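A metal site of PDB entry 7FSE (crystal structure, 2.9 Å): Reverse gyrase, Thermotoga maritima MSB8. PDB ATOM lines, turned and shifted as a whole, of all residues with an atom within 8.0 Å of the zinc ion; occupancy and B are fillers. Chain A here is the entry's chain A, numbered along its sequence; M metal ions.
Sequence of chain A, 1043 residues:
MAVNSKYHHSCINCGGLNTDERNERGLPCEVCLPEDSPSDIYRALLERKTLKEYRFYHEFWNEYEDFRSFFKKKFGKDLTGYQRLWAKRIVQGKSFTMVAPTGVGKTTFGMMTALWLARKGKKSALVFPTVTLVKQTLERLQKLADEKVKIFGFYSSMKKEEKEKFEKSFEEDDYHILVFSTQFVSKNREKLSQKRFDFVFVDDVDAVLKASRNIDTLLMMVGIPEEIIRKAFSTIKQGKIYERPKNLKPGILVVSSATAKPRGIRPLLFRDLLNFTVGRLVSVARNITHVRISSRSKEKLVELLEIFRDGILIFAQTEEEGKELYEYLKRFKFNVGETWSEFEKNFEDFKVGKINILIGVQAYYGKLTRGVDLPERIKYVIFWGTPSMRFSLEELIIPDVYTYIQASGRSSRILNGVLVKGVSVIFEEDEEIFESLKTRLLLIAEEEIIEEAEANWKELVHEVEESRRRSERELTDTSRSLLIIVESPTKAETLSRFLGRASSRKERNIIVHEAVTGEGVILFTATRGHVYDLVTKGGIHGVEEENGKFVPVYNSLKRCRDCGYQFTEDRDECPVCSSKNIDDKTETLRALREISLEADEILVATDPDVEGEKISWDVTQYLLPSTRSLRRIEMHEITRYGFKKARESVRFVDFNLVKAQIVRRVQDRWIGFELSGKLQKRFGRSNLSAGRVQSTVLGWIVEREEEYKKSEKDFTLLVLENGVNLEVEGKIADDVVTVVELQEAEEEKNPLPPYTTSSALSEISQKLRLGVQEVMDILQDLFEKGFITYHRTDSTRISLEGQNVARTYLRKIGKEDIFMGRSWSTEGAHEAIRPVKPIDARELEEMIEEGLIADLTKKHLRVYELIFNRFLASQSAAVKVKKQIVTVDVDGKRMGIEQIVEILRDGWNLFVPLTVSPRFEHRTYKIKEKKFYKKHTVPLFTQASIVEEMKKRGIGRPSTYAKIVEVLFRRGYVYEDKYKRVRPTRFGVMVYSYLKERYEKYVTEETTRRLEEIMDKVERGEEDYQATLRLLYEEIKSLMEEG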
ATOM      1  N   SER A  10      -2.488 -24.822   0.308  1.00  0.00           N
ATOM      2  CA  SER A  10      -1.186 -25.205  -0.205  1.00  0.00           C
ATOM      3  C   SER A  10      -0.470 -24.091  -0.963  1.00  0.00           C
ATOM      4  O   SER A  10       0.731 -24.218  -1.216  1.00  0.00           O
ATOM      5  CB  SER A  10      -1.312 -26.428  -1.115  1.00  0.00           C
ATOM      6  OG  SER A  10      -2.151 -26.159  -2.220  1.00  0.00           O
ATOM      7  N   CYS A  11      -1.159 -23.019  -1.339  1.00  0.00           N
ATOM      8  CA  CYS A  11      -0.488 -21.927  -2.043  1.00  0.00           C
ATOM      9  C   CYS A  11       0.524 -21.268  -1.131  1.00  0.00           C
ATOM     10  O   CYS A  11       0.199 -20.868  -0.006  1.00  0.00           O
ATOM     11  CB  CYS A  11      -1.506 -20.903  -2.548  1.00  0.00           C
ATOM     12  SG  CYS A  11      -0.742 -19.572  -3.524  1.00  0.00           S
ATOM     13  N   ILE A  12       1.756 -21.141  -1.618  1.00  0.00           N
ATOM     14  CA  ILE A  12       2.831 -20.627  -0.783  1.00  0.00           C
ATOM     15  C   ILE A  12       2.800 -19.101  -0.681  1.00  0.00           C
ATOM     16  O   ILE A  12       3.385 -18.538   0.246  1.00  0.00           O
ATOM     17  CB  ILE A  12       4.188 -21.111  -1.317  1.00  0.00           C
ATOM     18  CG1 ILE A  12       5.289 -20.902  -0.278  1.00  0.00           C
ATOM     19  CG2 ILE A  12       4.518 -20.434  -2.632  1.00  0.00           C
ATOM     20  CD1 ILE A  12       6.614 -21.507  -0.659  1.00  0.00           C
ATOM     21  N   ASN A  13       2.099 -18.418  -1.586  1.00  0.00           N
ATOM     22  CA  ASN A  13       2.067 -16.962  -1.600  1.00  0.00           C
ATOM     23  C   ASN A  13       0.805 -16.372  -0.991  1.00  0.00           C
ATOM     24  O   ASN A  13       0.891 -15.402  -0.228  1.00  0.00           O
ATOM     25  CB  ASN A  13       2.220 -16.438  -3.030  1.00  0.00           C
ATOM     26  CG  ASN A  13       2.123 -14.932  -3.102  1.00  0.00           C
ATOM     27  OD1 ASN A  13       3.046 -14.218  -2.722  1.00  0.00           O
ATOM     28  ND2 ASN A  13       0.984 -14.427  -3.578  1.00  0.00           N
ATOM     29  N   CYS A  14      -0.365 -16.910  -1.304  1.00  0.00           N
ATOM     30  CA  CYS A  14      -1.609 -16.377  -0.757  1.00  0.00           C
ATOM     31  C   CYS A  14      -2.204 -17.264   0.336  1.00  0.00           C
ATOM     32  O   CYS A  14      -3.173 -16.847   0.981  1.00  0.00           O
ATOM     33  CB  CYS A  14      -2.643 -16.158  -1.864  1.00  0.00           C
ATOM     34  SG  CYS A  14      -3.579 -17.626  -2.357  1.00  0.00           S
ATOM     35  N   GLY A  15      -1.652 -18.458   0.553  1.00  0.00           N
ATOM     36  CA  GLY A  15      -2.177 -19.334   1.575  1.00  0.00           C
ATOM     37  C   GLY A  15      -3.515 -19.952   1.257  1.00  0.00           C
ATOM     38  O   GLY A  15      -4.118 -20.591   2.130  1.00  0.00           O
ATOM     39  N   GLY A  16      -4.005 -19.797   0.027  1.00  0.00           N
ATOM     40  CA  GLY A  16      -5.299 -20.281  -0.382  1.00  0.00           C
ATOM     41  C   GLY A  16      -5.226 -21.603  -1.129  1.00  0.00           C
ATOM     42  O   GLY A  16      -4.314 -22.404  -0.915  1.00  0.00           O
ATOM     43  N   LEU A  17      -6.196 -21.821  -1.998  1.00  0.00           N
ATOM     44  CA  LEU A  17      -6.335 -23.088  -2.712  1.00  0.00           C
ATOM     45  C   LEU A  17      -5.462 -23.089  -3.959  1.00  0.00           C
ATOM     46  O   LEU A  17      -5.471 -22.119  -4.734  1.00  0.00           O
ATOM     47  CB  LEU A  17      -7.801 -23.325  -3.083  1.00  0.00           C
ATOM     48  CG  LEU A  17      -8.166 -24.597  -3.846  1.00  0.00           C
ATOM     49  CD1 LEU A  17      -9.416 -25.231  -3.256  1.00  0.00           C
ATOM     50  CD2 LEU A  17      -8.365 -24.303  -5.325  1.00  0.00           C
ATOM     51  N   ASN A  18      -4.721 -24.179  -4.159  1.00  0.00           N
ATOM     52  CA  ASN A  18      -3.895 -24.370  -5.340  1.00  0.00           C
ATOM     53  C   ASN A  18      -4.019 -25.817  -5.788  1.00  0.00           C
ATOM     54  O   ASN A  18      -4.314 -26.717  -4.993  1.00  0.00           O
ATOM     55  CB  ASN A  18      -2.427 -24.011  -5.078  1.00  0.00           C
ATOM     56  CG  ASN A  18      -1.577 -24.061  -6.327  1.00  0.00           C
ATOM     57  OD1 ASN A  18      -2.094 -24.055  -7.447  1.00  0.00           O
ATOM     58  ND2 ASN A  18      -0.259 -24.086  -6.152  1.00  0.00           N
ATOM     59  N   LEU A  27       4.968 -23.776  -7.997  1.00  0.00           N
ATOM     60  CA  LEU A  27       4.400 -22.476  -8.303  1.00  0.00           C
ATOM     61  C   LEU A  27       3.173 -22.188  -7.431  1.00  0.00           C
ATOM     62  O   LEU A  27       2.513 -23.107  -6.945  1.00  0.00           O
ATOM     63  CB  LEU A  27       3.980 -22.375  -9.780  1.00  0.00           C
ATOM     64  CG  LEU A  27       5.074 -22.095 -10.803  1.00  0.00           C
ATOM     65  CD1 LEU A  27       5.814 -23.364 -11.207  1.00  0.00           C
ATOM     66  CD2 LEU A  27       4.493 -21.385 -12.014  1.00  0.00           C
ATOM     67  N   PRO A  28       2.863 -20.901  -7.216  1.00  0.00           N
ATOM     68  CA  PRO A  28       1.610 -20.552  -6.524  1.00  0.00           C
ATOM     69  C   PRO A  28       0.383 -20.850  -7.363  1.00  0.00           C
ATOM     70  O   PRO A  28       0.489 -21.396  -8.466  1.00  0.00           O
ATOM     71  CB  PRO A  28       1.759 -19.048  -6.258  1.00  0.00           C
ATOM     72  CG  PRO A  28       3.238 -18.789  -6.349  1.00  0.00           C
ATOM     73  CD  PRO A  28       3.733 -19.733  -7.400  1.00  0.00           C
ATOM     74  N   CYS A  29      -0.793 -20.493  -6.859  1.00  0.00           N
ATOM     75  CA  CYS A  29      -2.036 -20.820  -7.535  1.00  0.00           C
ATOM     76  C   CYS A  29      -2.235 -19.944  -8.775  1.00  0.00           C
ATOM     77  O   CYS A  29      -1.496 -18.991  -9.025  1.00  0.00           O
ATOM     78  CB  CYS A  29      -3.224 -20.686  -6.585  1.00  0.00           C
ATOM     79  SG  CYS A  29      -3.549 -18.999  -6.011  1.00  0.00           S
ATOM     80  N   GLU A  30      -3.273 -20.279  -9.550  1.00  0.00           N
ATOM     81  CA  GLU A  30      -3.565 -19.528 -10.757  1.00  0.00           C
ATOM     82  C   GLU A  30      -3.911 -18.079 -10.445  1.00  0.00           C
ATOM     83  O   GLU A  30      -3.591 -17.171 -11.224  1.00  0.00           O
ATOM     84  CB  GLU A  30      -4.720 -20.193 -11.513  1.00  0.00           C
ATOM     85  CG  GLU A  30      -4.576 -20.168 -13.030  1.00  0.00           C
ATOM     86  CD  GLU A  30      -3.923 -21.429 -13.582  1.00  0.00           C
ATOM     87  OE1 GLU A  30      -4.487 -22.526 -13.371  1.00  0.00           O
ATOM     88  OE2 GLU A  30      -2.849 -21.327 -14.196  1.00  0.00           O
ATOM     89  N   VAL A  31      -4.569 -17.830  -9.308  1.00  0.00           N
ATOM     90  CA  VAL A  31      -4.969 -16.480  -8.946  1.00  0.00           C
ATOM     91  C   VAL A  31      -3.749 -15.589  -8.727  1.00  0.00           C
ATOM     92  O   VAL A  31      -3.700 -14.445  -9.185  1.00  0.00           O
ATOM     93  CB  VAL A  31      -5.874 -16.507  -7.692  1.00  0.00           C
ATOM     94  CG1 VAL A  31      -6.331 -15.103  -7.330  1.00  0.00           C
ATOM     95  CG2 VAL A  31      -7.065 -17.424  -7.925  1.00  0.00           C
ATOM     96  N   CYS A  32      -2.736 -16.114  -8.028  1.00  0.00           N
ATOM     97  CA  CYS A  32      -1.551 -15.306  -7.734  1.00  0.00           C
ATOM     98  C   CYS A  32      -0.731 -15.042  -8.989  1.00  0.00           C
ATOM     99  O   CYS A  32      -0.318 -13.904  -9.251  1.00  0.00           O
ATOM    100  CB  CYS A  32      -0.703 -15.998  -6.672  1.00  0.00           C
ATOM    101  SG  CYS A  32      -1.441 -16.041  -5.021  1.00  0.00           S
ATOM    102  N   LEU A  33      -0.484 -16.085  -9.784  1.00  0.00           N
ATOM    103  CA  LEU A  33       0.405 -15.973 -10.940  1.00  0.00           C
ATOM    104  C   LEU A  33      -0.076 -16.940 -12.014  1.00  0.00           C
ATOM    105  O   LEU A  33       0.187 -18.147 -11.952  1.00  0.00           O
ATOM    106  CB  LEU A  33       1.849 -16.272 -10.549  1.00  0.00           C
ATOM    107  CG  LEU A  33       2.866 -16.269 -11.688  1.00  0.00           C
ATOM    108  CD1 LEU A  33       2.787 -14.971 -12.470  1.00  0.00           C
ATOM    109  CD2 LEU A  33       4.258 -16.504 -11.152  1.00  0.00           C
ATOM    110  N   LEU A  45       5.204 -12.077  -9.232  1.00  0.00           N
ATOM    111  CA  LEU A  45       4.229 -11.702  -8.210  1.00  0.00           C
ATOM    112  C   LEU A  45       4.307 -10.212  -7.890  1.00  0.00           C
ATOM    113  O   LEU A  45       3.275  -9.576  -7.656  1.00  0.00           O
ATOM    114  CB  LEU A  45       4.440 -12.543  -6.952  1.00  0.00           C
ATOM    115  CG  LEU A  45       3.989 -13.995  -7.044  1.00  0.00           C
ATOM    116  CD1 LEU A  45       4.647 -14.833  -5.956  1.00  0.00           C
ATOM    117  CD2 LEU A  45       2.474 -14.073  -6.917  1.00  0.00           C
ATOM    118  N   THR A  50       0.478  -8.948  -6.499  1.00  0.00           N
ATOM    119  CA  THR A  50      -0.137 -10.006  -5.710  1.00  0.00           C
ATOM    120  C   THR A  50       0.835 -10.591  -4.693  1.00  0.00           C
ATOM    121  O   THR A  50       0.559 -11.656  -4.123  1.00  0.00           O
ATOM    122  CB  THR A  50      -0.663 -11.109  -6.616  1.00  0.00           C
ATOM    123  OG1 THR A  50       0.383 -11.561  -7.483  1.00  0.00           O
ATOM    124  CG2 THR A  50      -1.825 -10.604  -7.461  1.00  0.00           C
ATOM    125  N   LYS A  52       2.252 -11.368  -1.449  1.00  0.00           N
ATOM    126  CA  LYS A  52       1.830 -11.311  -0.052  1.00  0.00           C
ATOM    127  C   LYS A  52       2.761 -12.064   0.886  1.00  0.00           C
ATOM    128  O   LYS A  52       3.316 -11.457   1.813  1.00  0.00           O
ATOM    129  CB  LYS A  52       0.396 -11.842   0.067  1.00  0.00           C
ATOM    130  CG  LYS A  52      -0.577 -11.168  -0.896  1.00  0.00           C
ATOM    131  CD  LYS A  52      -1.795 -12.032  -1.125  1.00  0.00           C
ATOM    132  CE  LYS A  52      -2.558 -11.576  -2.356  1.00  0.00           C
ATOM    133  NZ  LYS A  52      -3.617 -12.542  -2.748  1.00  0.00           N
HETATM  134 ZN    ZN M   1      -2.326 -18.049  -4.264  1.00  0.00          ZN
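The zinc ion is bound by the side-chain sulfur of Cys 11 (2.3 Å), the side-chain sulfur of Cys 14 (2.3 Å), the side-chain sulfur of Cys 32 (2.3 Å) and the side-chain sulfur of Cys 29 (2.3 Å). The zinc ion has four donor atoms within binding distance.
The backbone NH (N) of Asn 13 lies close to the side-chain sulfur (SG) of Cys 11. The backbone NH (N) of Cys 11 sits at hydrogen-bond distance from the backbone carbonyl oxygen (O) of Gly 16. N of Val 31 sits close to SG of Cys 29. The backbone NH of Gly 16 lies close to the side-chain sulfur of Cys 14. The side-chain sulfur of Cys 32 lies close to the side-chain amide nitrogen of Asn 13 (3.3 Å). The side-chain hydroxyl (OG1) of Thr 50 lies within hydrogen-bond range of the backbone carbonyl oxygen (O) of Cys 32, at 3.0 Å.
Of the 19 residues printed, 4 come within 4 Å of the zinc ion.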
